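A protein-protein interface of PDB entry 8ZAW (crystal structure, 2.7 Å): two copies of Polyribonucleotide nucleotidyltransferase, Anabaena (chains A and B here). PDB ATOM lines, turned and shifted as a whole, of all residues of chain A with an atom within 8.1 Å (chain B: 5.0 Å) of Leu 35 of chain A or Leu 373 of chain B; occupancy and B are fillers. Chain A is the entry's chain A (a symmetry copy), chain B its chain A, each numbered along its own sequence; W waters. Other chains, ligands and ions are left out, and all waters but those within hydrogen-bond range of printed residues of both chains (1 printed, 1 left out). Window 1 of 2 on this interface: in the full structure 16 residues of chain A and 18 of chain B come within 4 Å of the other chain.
The side-chain amide nitrogen of Gln 371 of chain B lies within hydrogen-bond range of the backbone carbonyl oxygen of Leu 34 of chain A (3.0 Å).
OE1 of Gln 371 of chain B is in hydrogen-bond range of N of Ala 36 of chain A, 2.4 Å away.
OE2 of Glu 453 of chain B is in hydrogen-bond range of OH of Tyr 79 of chain A (2.6 Å).
O of Gln 371 of chain B sits at hydrogen-bond distance from N of Leu 455 of chain B, 3.0 Å away.
The backbone carbonyl oxygen of Leu 373 of chain B lies within hydrogen-bond range of the backbone NH of Glu 453 of chain B (2.8 Å).
N of Ala 375 of chain B lies within hydrogen-bond range of O of Val 451 of chain B (2.9 Å).
N of Leu 44 of chain A sits at hydrogen-bond distance from O of Lys 31 of chain A (3.0 Å).
O of Leu 35 of chain A is in hydrogen-bond range of OG of Ser 42 of chain A, at 2.8 Å.
The backbone NH (N) of Leu 53 of chain A is in hydrogen-bond range of the backbone carbonyl oxygen (O) of Leu 127 of chain A (2.8 Å).
Among the printed residues, pairs that only touch across the chains: Pro 37 of chain A with Gln 371 of chain B, Leu 35 of chain A with Gln 371 of chain B, Leu 35 of chain A with Leu 364 of chain B, Leu 127 of chain A with Glu 453 of chain B, Leu 35 of chain A with Leu 455 of chain B, Tyr 79 of chain A with Val 451 of chain B, Tyr 79 of chain A with Ala 375 of chain B, Lys 31 of chain A with Val 354 of chain B, Ala 36 of chain A with Leu 455 of chain B, Leu 35 of chain A with Leu 373 of chain B and Met 129 of chain A with Leu 355 of chain B.
Of the printed residues of chain B, Lys 31 of chain A touches Val 354.
Of chain B, only Leu 364 (3.5 Å), Gln 371 (3.2 Å), Leu 373 (3.8 Å) and Leu 455 (3.6 Å) come within 4 Å of Leu 35 of chain A.
Of the printed residues of chain B, Pro 37 of chain A touches Gln 371.
Val 43 of chain A touches none of the printed residues of chain B.
Leu 373 of chain B touches just one residue of chain A: Leu 35 (3.8 Å).
Printed residues of chain A within 4 Å of Val 451 of chain B: Tyr 79 (3.6 Å).
Of the 13 printed residues of chain B, 9 touch a printed residue of chain A.
Hydrophobic or aromatic side chains of chain B within 4 Å of the printed part of chain A: Leu 355, Leu 364, Leu 373, Ala 375, Val 451 and Leu 455.
Hydrophobic or aromatic side chains of chain A that line the printed part of chain B: Leu 35, Ala 36, Pro 37, Tyr 79, Leu 127 and Met 129.
Among the printed residues, no Asp or Glu carboxylate lies within 4 Å of a Lys or Arg side-chain nitrogen of the other chain.
No position is printed for both chains.
Of the 14 pairs that touch across the chains among the printed residues, none has its exchanged pair printed and touching as well.
Water W1 lies within hydrogen-bond range of the backbone NH (N) of Gln 38 of chain A (2.9 Å), the backbone carbonyl oxygen (O) of Leu 455 of chain B (3.0 Å) and the backbone NH (N) of Ala 39 of chain A (3.1 Å).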
ATOM      1  N   ALA A  15      -6.642 -37.587 -14.622  1.00  0.00           N
ATOM      2  CA  ALA A  15      -6.525 -37.656 -13.163  1.00  0.00           C
ATOM      3  C   ALA A  15      -5.187 -37.071 -12.713  1.00  0.00           C
ATOM      4  O   ALA A  15      -4.355 -36.715 -13.543  1.00  0.00           O
ATOM      5  CB  ALA A  15      -6.679 -39.081 -12.679  1.00  0.00           C
ATOM      6  N   GLU A  16      -4.972 -36.976 -11.406  1.00  0.00           N
ATOM      7  CA  GLU A  16      -3.910 -36.130 -10.884  1.00  0.00           C
ATOM      8  C   GLU A  16      -2.586 -36.882 -10.741  1.00  0.00           C
ATOM      9  O   GLU A  16      -2.539 -38.078 -10.431  1.00  0.00           O
ATOM     10  CB  GLU A  16      -4.327 -35.522  -9.548  1.00  0.00           C
ATOM     11  CG  GLU A  16      -4.488 -36.523  -8.447  1.00  0.00           C
ATOM     12  CD  GLU A  16      -5.818 -37.237  -8.525  1.00  0.00           C
ATOM     13  OE1 GLU A  16      -6.696 -36.816  -9.317  1.00  0.00           O
ATOM     14  OE2 GLU A  16      -5.971 -38.240  -7.805  1.00  0.00           O
ATOM     15  N   LYS A  31       1.794 -30.429 -10.335  1.00  0.00           N
ATOM     16  CA  LYS A  31       0.603 -31.263 -10.266  1.00  0.00           C
ATOM     17  C   LYS A  31      -0.181 -31.075 -11.558  1.00  0.00           C
ATOM     18  O   LYS A  31      -0.646 -29.969 -11.848  1.00  0.00           O
ATOM     19  CB  LYS A  31      -0.247 -30.928  -9.035  1.00  0.00           C
ATOM     20  CG  LYS A  31       0.467 -31.169  -7.690  1.00  0.00           C
ATOM     21  CD  LYS A  31      -0.498 -31.319  -6.506  1.00  0.00           C
ATOM     22  CE  LYS A  31      -1.062 -29.978  -6.014  1.00  0.00           C
ATOM     23  NZ  LYS A  31      -1.952 -30.124  -4.808  1.00  0.00           N
ATOM     24  N   VAL A  32      -0.297 -32.149 -12.344  1.00  0.00           N
ATOM     25  CA  VAL A  32      -1.069 -32.166 -13.577  1.00  0.00           C
ATOM     26  C   VAL A  32      -2.253 -33.116 -13.382  1.00  0.00           C
ATOM     27  O   VAL A  32      -2.211 -34.048 -12.570  1.00  0.00           O
ATOM     28  CB  VAL A  32      -0.220 -32.585 -14.813  1.00  0.00           C
ATOM     29  CG1 VAL A  32       1.057 -31.744 -14.938  1.00  0.00           C
ATOM     30  CG2 VAL A  32       0.133 -34.050 -14.760  1.00  0.00           C
ATOM     31  N   GLY A  33      -3.325 -32.867 -14.140  1.00  0.00           N
ATOM     32  CA  GLY A  33      -4.524 -33.681 -14.036  1.00  0.00           C
ATOM     33  C   GLY A  33      -5.419 -33.364 -12.862  1.00  0.00           C
ATOM     34  O   GLY A  33      -6.404 -34.078 -12.631  1.00  0.00           O
ATOM     35  N   LEU A  34      -5.109 -32.302 -12.119  1.00  0.00           N
ATOM     36  CA  LEU A  34      -5.826 -31.880 -10.927  1.00  0.00           C
ATOM     37  C   LEU A  34      -6.874 -30.804 -11.213  1.00  0.00           C
ATOM     38  O   LEU A  34      -8.048 -30.979 -10.861  1.00  0.00           O
ATOM     39  CB  LEU A  34      -4.816 -31.385  -9.886  1.00  0.00           C
ATOM     40  CG  LEU A  34      -5.359 -30.936  -8.526  1.00  0.00           C
ATOM     41  CD1 LEU A  34      -5.937 -32.112  -7.752  1.00  0.00           C
ATOM     42  CD2 LEU A  34      -4.271 -30.281  -7.705  1.00  0.00           C
ATOM     43  N   LEU A  35      -6.492 -29.706 -11.875  1.00  0.00           N
ATOM     44  CA  LEU A  35      -7.323 -28.510 -11.979  1.00  0.00           C
ATOM     45  C   LEU A  35      -7.457 -28.036 -13.425  1.00  0.00           C
ATOM     46  O   LEU A  35      -6.571 -28.250 -14.252  1.00  0.00           O
ATOM     47  CB  LEU A  35      -6.742 -27.382 -11.121  1.00  0.00           C
ATOM     48  CG  LEU A  35      -6.751 -27.625  -9.610  1.00  0.00           C
ATOM     49  CD1 LEU A  35      -6.036 -26.492  -8.884  1.00  0.00           C
ATOM     50  CD2 LEU A  35      -8.165 -27.757  -9.108  1.00  0.00           C
ATOM     51  N   ALA A  36      -8.579 -27.370 -13.715  1.00  0.00           N
ATOM     52  CA  ALA A  36      -8.948 -26.817 -15.025  1.00  0.00           C
ATOM     53  C   ALA A  36      -8.984 -27.886 -16.111  1.00  0.00           C
ATOM     54  O   ALA A  36      -8.122 -27.900 -17.000  1.00  0.00           O
ATOM     55  CB  ALA A  36      -7.986 -25.697 -15.432  1.00  0.00           C
ATOM     56  N   PRO A  37      -9.964 -28.792 -16.082  1.00  0.00           N
ATOM     57  CA  PRO A  37      -9.943 -29.931 -17.012  1.00  0.00           C
ATOM     58  C   PRO A  37     -10.374 -29.597 -18.439  1.00  0.00           C
ATOM     59  O   PRO A  37     -10.203 -30.441 -19.334  1.00  0.00           O
ATOM     60  CB  PRO A  37     -10.902 -30.936 -16.354  1.00  0.00           C
ATOM     61  CG  PRO A  37     -11.809 -30.103 -15.513  1.00  0.00           C
ATOM     62  CD  PRO A  37     -11.050 -28.895 -15.090  1.00  0.00           C
ATOM     63  N   GLN A  38     -10.890 -28.402 -18.693  1.00  0.00           N
ATOM     64  CA  GLN A  38     -11.162 -27.984 -20.058  1.00  0.00           C
ATOM     65  C   GLN A  38     -10.024 -27.180 -20.673  1.00  0.00           C
ATOM     66  O   GLN A  38     -10.149 -26.733 -21.812  1.00  0.00           O
ATOM     67  CB  GLN A  38     -12.456 -27.173 -20.102  1.00  0.00           C
ATOM     68  CG  GLN A  38     -13.700 -28.036 -20.098  1.00  0.00           C
ATOM     69  CD  GLN A  38     -14.969 -27.229 -20.289  1.00  0.00           C
ATOM     70  OE1 GLN A  38     -15.800 -27.104 -19.369  1.00  0.00           O
ATOM     71  NE2 GLN A  38     -15.138 -26.681 -21.491  1.00  0.00           N
ATOM     72  N   ALA A  39      -8.923 -26.981 -19.965  1.00  0.00           N
ATOM     73  CA  ALA A  39      -7.770 -26.313 -20.551  1.00  0.00           C
ATOM     74  C   ALA A  39      -6.941 -27.279 -21.395  1.00  0.00           C
ATOM     75  O   ALA A  39      -6.825 -28.470 -21.079  1.00  0.00           O
ATOM     76  CB  ALA A  39      -6.889 -25.708 -19.456  1.00  0.00           C
ATOM     77  N   GLY A  41      -3.698 -27.384 -21.498  1.00  0.00           N
ATOM     78  CA  GLY A  41      -2.751 -27.923 -20.528  1.00  0.00           C
ATOM     79  C   GLY A  41      -2.758 -27.117 -19.245  1.00  0.00           C
ATOM     80  O   GLY A  41      -3.055 -25.917 -19.255  1.00  0.00           O
ATOM     81  N   SER A  42      -2.422 -27.775 -18.126  1.00  0.00           N
ATOM     82  CA  SER A  42      -2.457 -27.112 -16.818  1.00  0.00           C
ATOM     83  C   SER A  42      -1.502 -27.766 -15.813  1.00  0.00           C
ATOM     84  O   SER A  42      -1.252 -28.971 -15.864  1.00  0.00           O
ATOM     85  CB  SER A  42      -3.879 -27.110 -16.218  1.00  0.00           C
ATOM     86  OG  SER A  42      -4.320 -28.414 -15.855  1.00  0.00           O
ATOM     87  N   VAL A  43      -1.010 -26.961 -14.868  1.00  0.00           N
ATOM     88  CA  VAL A  43      -0.193 -27.431 -13.750  1.00  0.00           C
ATOM     89  C   VAL A  43      -0.394 -26.489 -12.577  1.00  0.00           C
ATOM     90  O   VAL A  43      -0.490 -25.273 -12.754  1.00  0.00           O
ATOM     91  CB  VAL A  43       1.311 -27.517 -14.113  1.00  0.00           C
ATOM     92  CG1 VAL A  43       1.946 -26.140 -14.278  1.00  0.00           C
ATOM     93  CG2 VAL A  43       2.079 -28.293 -13.108  1.00  0.00           C
ATOM     94  N   LEU A  44      -0.526 -27.053 -11.379  1.00  0.00           N
ATOM     95  CA  LEU A  44      -0.123 -26.351 -10.154  1.00  0.00           C
ATOM     96  C   LEU A  44       1.349 -26.524  -9.953  1.00  0.00           C
ATOM     97  O   LEU A  44       1.790 -27.586  -9.518  1.00  0.00           O
ATOM     98  CB  LEU A  44      -0.833 -26.818  -8.884  1.00  0.00           C
ATOM     99  CG  LEU A  44      -2.148 -26.241  -8.449  1.00  0.00           C
ATOM    100  CD1 LEU A  44      -2.602 -27.047  -7.270  1.00  0.00           C
ATOM    101  CD2 LEU A  44      -1.843 -24.813  -7.942  1.00  0.00           C
ATOM    102  N   GLU A  46       4.389 -25.455  -7.611  1.00  0.00           N
ATOM    103  CA  GLU A  46       4.496 -25.139  -6.196  1.00  0.00           C
ATOM    104  C   GLU A  46       5.959 -25.188  -5.777  1.00  0.00           C
ATOM    105  O   GLU A  46       6.714 -26.051  -6.233  1.00  0.00           O
ATOM    106  CB  GLU A  46       3.715 -26.140  -5.350  1.00  0.00           C
ATOM    107  CG  GLU A  46       2.231 -26.206  -5.602  1.00  0.00           C
ATOM    108  CD  GLU A  46       1.561 -27.258  -4.735  1.00  0.00           C
ATOM    109  OE1 GLU A  46       2.145 -28.347  -4.541  1.00  0.00           O
ATOM    110  OE2 GLU A  46       0.471 -26.972  -4.203  1.00  0.00           O
ATOM    111  N   VAL A  52       1.067 -21.597  -7.711  1.00  0.00           N
ATOM    112  CA  VAL A  52       0.446 -20.845  -8.787  1.00  0.00           C
ATOM    113  C   VAL A  52      -0.055 -21.834  -9.827  1.00  0.00           C
ATOM    114  O   VAL A  52       0.640 -22.802 -10.162  1.00  0.00           O
ATOM    115  CB  VAL A  52       1.398 -19.773  -9.382  1.00  0.00           C
ATOM    116  CG1 VAL A  52       2.701 -20.336  -9.757  1.00  0.00           C
ATOM    117  CG2 VAL A  52       0.791 -19.110 -10.605  1.00  0.00           C
ATOM    118  N   LEU A  53      -1.289 -21.617 -10.285  1.00  0.00           N
ATOM    119  CA  LEU A  53      -1.934 -22.455 -11.286  1.00  0.00           C
ATOM    120  C   LEU A  53      -1.803 -21.803 -12.658  1.00  0.00           C
ATOM    121  O   LEU A  53      -2.181 -20.636 -12.841  1.00  0.00           O
ATOM    122  CB  LEU A  53      -3.409 -22.662 -10.943  1.00  0.00           C
ATOM    123  CG  LEU A  53      -4.227 -23.232 -12.116  1.00  0.00           C
ATOM    124  CD1 LEU A  53      -3.702 -24.620 -12.570  1.00  0.00           C
ATOM    125  CD2 LEU A  53      -5.746 -23.234 -11.873  1.00  0.00           C
ATOM    126  N   VAL A  54      -1.293 -22.560 -13.628  1.00  0.00           N
ATOM    127  CA  VAL A  54      -0.987 -22.035 -14.958  1.00  0.00           C
ATOM    128  C   VAL A  54      -1.645 -22.927 -16.011  1.00  0.00           C
ATOM    129  O   VAL A  54      -1.305 -24.113 -16.132  1.00  0.00           O
ATOM    130  CB  VAL A  54       0.535 -21.940 -15.183  1.00  0.00           C
ATOM    131  CG1 VAL A  54       0.839 -21.222 -16.460  1.00  0.00           C
ATOM    132  CG2 VAL A  54       1.213 -21.231 -14.006  1.00  0.00           C
ATOM    133  N   THR A  55      -2.577 -22.358 -16.779  1.00  0.00           N
ATOM    134  CA  THR A  55      -3.271 -23.074 -17.848  1.00  0.00           C
ATOM    135  C   THR A  55      -2.907 -22.470 -19.193  1.00  0.00           C
ATOM    136  O   THR A  55      -2.441 -21.334 -19.271  1.00  0.00           O
ATOM    137  CB  THR A  55      -4.806 -23.011 -17.715  1.00  0.00           C
ATOM    138  OG1 THR A  55      -5.261 -21.676 -18.021  1.00  0.00           O
ATOM    139  CG2 THR A  55      -5.228 -23.400 -16.323  1.00  0.00           C
ATOM    140  N   TYR A  79      -6.664 -13.902  -1.077  1.00  0.00           N
ATOM    141  CA  TYR A  79      -6.813 -15.031  -0.167  1.00  0.00           C
ATOM    142  C   TYR A  79      -5.537 -15.847  -0.059  1.00  0.00           C
ATOM    143  O   TYR A  79      -5.357 -16.570   0.922  1.00  0.00           O
ATOM    144  CB  TYR A  79      -7.977 -15.921  -0.594  1.00  0.00           C
ATOM    145  CG  TYR A  79      -7.849 -16.614  -1.936  1.00  0.00           C
ATOM    146  CD1 TYR A  79      -6.973 -17.682  -2.118  1.00  0.00           C
ATOM    147  CD2 TYR A  79      -8.644 -16.229  -3.018  1.00  0.00           C
ATOM    148  CE1 TYR A  79      -6.870 -18.323  -3.336  1.00  0.00           C
ATOM    149  CE2 TYR A  79      -8.549 -16.862  -4.238  1.00  0.00           C
ATOM    150  CZ  TYR A  79      -7.654 -17.906  -4.399  1.00  0.00           C
ATOM    151  OH  TYR A  79      -7.563 -18.541  -5.626  1.00  0.00           O
ATOM    152  N   LEU A 127      -2.888 -17.931 -12.068  1.00  0.00           N
ATOM    153  CA  LEU A 127      -3.420 -17.457 -10.792  1.00  0.00           C
ATOM    154  C   LEU A 127      -2.497 -17.907  -9.672  1.00  0.00           C
ATOM    155  O   LEU A 127      -2.307 -19.108  -9.467  1.00  0.00           O
ATOM    156  CB  LEU A 127      -4.828 -17.989 -10.521  1.00  0.00           C
ATOM    157  CG  LEU A 127      -5.925 -17.888 -11.565  1.00  0.00           C
ATOM    158  CD1 LEU A 127      -7.128 -18.686 -11.073  1.00  0.00           C
ATOM    159  CD2 LEU A 127      -6.290 -16.444 -11.829  1.00  0.00           C
ATOM    160  N   MET A 129      -2.198 -18.728  -6.026  1.00  0.00           N
ATOM    161  CA  MET A 129      -3.201 -19.161  -5.070  1.00  0.00           C
ATOM    162  C   MET A 129      -2.664 -19.377  -3.661  1.00  0.00           C
ATOM    163  O   MET A 129      -3.464 -19.619  -2.748  1.00  0.00           O
ATOM    164  CB  MET A 129      -3.862 -20.438  -5.578  1.00  0.00           C
ATOM    165  CG  MET A 129      -4.321 -20.298  -7.016  1.00  0.00           C
ATOM    166  SD  MET A 129      -5.206 -21.748  -7.601  1.00  0.00           S
ATOM    167  CE  MET A 129      -6.668 -20.975  -8.273  1.00  0.00           C
ATOM    168  N   VAL B 354      -6.793 -28.684  -0.644  1.00  0.00           N
ATOM    169  CA  VAL B 354      -6.075 -28.668  -1.914  1.00  0.00           C
ATOM    170  C   VAL B 354      -4.905 -27.695  -1.874  1.00  0.00           C
ATOM    171  O   VAL B 354      -3.863 -27.928  -2.503  1.00  0.00           O
ATOM    172  CB  VAL B 354      -7.051 -28.334  -3.065  1.00  0.00           C
ATOM    173  CG1 VAL B 354      -7.781 -27.019  -2.824  1.00  0.00           C
ATOM    174  CG2 VAL B 354      -6.329 -28.324  -4.409  1.00  0.00           C
ATOM    175  N   LEU B 355      -5.050 -26.599  -1.147  1.00  0.00           N
ATOM    176  CA  LEU B 355      -4.022 -25.584  -1.039  1.00  0.00           C
ATOM    177  C   LEU B 355      -3.330 -25.681   0.307  1.00  0.00           C
ATOM    178  O   LEU B 355      -3.833 -26.338   1.227  1.00  0.00           O
ATOM    179  CB  LEU B 355      -4.647 -24.194  -1.218  1.00  0.00           C
ATOM    180  CG  LEU B 355      -5.081 -23.988  -2.668  1.00  0.00           C
ATOM    181  CD1 LEU B 355      -5.999 -22.803  -2.816  1.00  0.00           C
ATOM    182  CD2 LEU B 355      -3.864 -23.835  -3.565  1.00  0.00           C
ATOM    183  N   GLY B 363     -11.254 -26.070  -0.765  1.00  0.00           N
ATOM    184  CA  GLY B 363     -12.176 -27.093  -1.219  1.00  0.00           C
ATOM    185  C   GLY B 363     -12.317 -27.146  -2.725  1.00  0.00           C
ATOM    186  O   GLY B 363     -12.625 -26.132  -3.354  1.00  0.00           O
ATOM    187  N   LEU B 364     -12.102 -28.313  -3.315  1.00  0.00           N
ATOM    188  CA  LEU B 364     -12.284 -28.515  -4.749  1.00  0.00           C
ATOM    189  C   LEU B 364     -13.506 -29.392  -4.990  1.00  0.00           C
ATOM    190  O   LEU B 364     -13.598 -30.486  -4.432  1.00  0.00           O
ATOM    191  CB  LEU B 364     -11.045 -29.172  -5.371  1.00  0.00           C
ATOM    192  CG  LEU B 364     -11.129 -29.490  -6.869  1.00  0.00           C
ATOM    193  CD1 LEU B 364     -11.273 -28.212  -7.668  1.00  0.00           C
ATOM    194  CD2 LEU B 364      -9.953 -30.287  -7.359  1.00  0.00           C
ATOM    195  N   GLN B 371     -15.879 -27.417 -12.485  1.00  0.00           N
ATOM    196  CA  GLN B 371     -14.893 -27.486 -11.411  1.00  0.00           C
ATOM    197  C   GLN B 371     -14.836 -26.133 -10.700  1.00  0.00           C
ATOM    198  O   GLN B 371     -14.792 -25.081 -11.348  1.00  0.00           O
ATOM    199  CB  GLN B 371     -13.516 -27.884 -11.986  1.00  0.00           C
ATOM    200  CG  GLN B 371     -12.455 -28.279 -10.973  1.00  0.00           C
ATOM    201  CD  GLN B 371     -11.139 -28.698 -11.628  1.00  0.00           C
ATOM    202  OE1 GLN B 371     -10.478 -27.901 -12.278  1.00  0.00           O
ATOM    203  NE2 GLN B 371     -10.753 -29.948 -11.435  1.00  0.00           N
ATOM    204  N   VAL B 372     -14.859 -26.149  -9.373  1.00  0.00           N
ATOM    205  CA  VAL B 372     -14.804 -24.924  -8.584  1.00  0.00           C
ATOM    206  C   VAL B 372     -13.842 -25.149  -7.425  1.00  0.00           C
ATOM    207  O   VAL B 372     -13.885 -26.194  -6.768  1.00  0.00           O
ATOM    208  CB  VAL B 372     -16.195 -24.510  -8.066  1.00  0.00           C
ATOM    209  CG1 VAL B 372     -16.093 -23.242  -7.248  1.00  0.00           C
ATOM    210  CG2 VAL B 372     -17.203 -24.329  -9.226  1.00  0.00           C
ATOM    211  N   LEU B 373     -12.954 -24.195  -7.194  1.00  0.00           N
ATOM    212  CA  LEU B 373     -12.044 -24.266  -6.061  1.00  0.00           C
ATOM    213  C   LEU B 373     -12.370 -23.123  -5.110  1.00  0.00           C
ATOM    214  O   LEU B 373     -12.240 -21.952  -5.472  1.00  0.00           O
ATOM    215  CB  LEU B 373     -10.581 -24.223  -6.517  1.00  0.00           C
ATOM    216  CG  LEU B 373      -9.566 -24.694  -5.459  1.00  0.00           C
ATOM    217  CD1 LEU B 373      -8.232 -25.160  -6.070  1.00  0.00           C
ATOM    218  CD2 LEU B 373      -9.324 -23.597  -4.420  1.00  0.00           C
ATOM    219  N   SER B 374     -12.787 -23.457  -3.901  1.00  0.00           N
ATOM    220  CA  SER B 374     -13.190 -22.449  -2.930  1.00  0.00           C
ATOM    221  C   SER B 374     -12.087 -22.231  -1.908  1.00  0.00           C
ATOM    222  O   SER B 374     -11.408 -23.177  -1.489  1.00  0.00           O
ATOM    223  CB  SER B 374     -14.486 -22.834  -2.205  1.00  0.00           C
ATOM    224  OG  SER B 374     -15.617 -22.628  -3.034  1.00  0.00           O
ATOM    225  N   ALA B 375     -11.915 -20.980  -1.518  1.00  0.00           N
ATOM    226  CA  ALA B 375     -10.851 -20.609  -0.606  1.00  0.00           C
ATOM    227  C   ALA B 375     -11.448 -19.764   0.503  1.00  0.00           C
ATOM    228  O   ALA B 375     -12.280 -18.888   0.253  1.00  0.00           O
ATOM    229  CB  ALA B 375      -9.734 -19.856  -1.325  1.00  0.00           C
ATOM    230  N   VAL B 451     -13.819 -17.168  -1.605  1.00  0.00           N
ATOM    231  CA  VAL B 451     -13.598 -16.917  -3.021  1.00  0.00           C
ATOM    232  C   VAL B 451     -13.765 -18.236  -3.759  1.00  0.00           C
ATOM    233  O   VAL B 451     -13.110 -19.226  -3.422  1.00  0.00           O
ATOM    234  CB  VAL B 451     -12.207 -16.303  -3.289  1.00  0.00           C
ATOM    235  CG1 VAL B 451     -12.022 -16.040  -4.773  1.00  0.00           C
ATOM    236  CG2 VAL B 451     -12.022 -15.022  -2.486  1.00  0.00           C
ATOM    237  N   SER B 452     -14.647 -18.250  -4.743  1.00  0.00           N
ATOM    238  CA  SER B 452     -14.876 -19.403  -5.609  1.00  0.00           C
ATOM    239  C   SER B 452     -14.187 -19.154  -6.947  1.00  0.00           C
ATOM    240  O   SER B 452     -14.616 -18.299  -7.726  1.00  0.00           O
ATOM    241  CB  SER B 452     -16.373 -19.648  -5.802  1.00  0.00           C
ATOM    242  OG  SER B 452     -16.934 -20.269  -4.655  1.00  0.00           O
ATOM    243  N   GLU B 453     -13.114 -19.888  -7.205  1.00  0.00           N
ATOM    244  CA  GLU B 453     -12.448 -19.865  -8.500  1.00  0.00           C
ATOM    245  C   GLU B 453     -13.136 -20.885  -9.391  1.00  0.00           C
ATOM    246  O   GLU B 453     -13.078 -22.090  -9.119  1.00  0.00           O
ATOM    247  CB  GLU B 453     -10.965 -20.183  -8.349  1.00  0.00           C
ATOM    248  CG  GLU B 453     -10.232 -19.240  -7.416  1.00  0.00           C
ATOM    249  CD  GLU B 453      -9.697 -18.008  -8.128  1.00  0.00           C
ATOM    250  OE1 GLU B 453     -10.059 -17.780  -9.312  1.00  0.00           O
ATOM    251  OE2 GLU B 453      -8.917 -17.265  -7.497  1.00  0.00           O
ATOM    252  N   LEU B 455     -12.940 -22.933 -12.361  1.00  0.00           N
ATOM    253  CA  LEU B 455     -11.827 -23.361 -13.206  1.00  0.00           C
ATOM    254  C   LEU B 455     -12.285 -24.079 -14.462  1.00  0.00           C
ATOM    255  O   LEU B 455     -11.528 -24.145 -15.439  1.00  0.00           O
ATOM    256  CB  LEU B 455     -10.861 -24.267 -12.414  1.00  0.00           C
ATOM    257  CG  LEU B 455     -10.395 -23.702 -11.056  1.00  0.00           C
ATOM    258  CD1 LEU B 455      -9.519 -24.672 -10.279  1.00  0.00           C
ATOM    259  CD2 LEU B 455      -9.665 -22.388 -11.249  1.00  0.00           C
HETATM  260  O   HOH W   1     -10.742 -25.690 -17.826  1.00  0.00           O
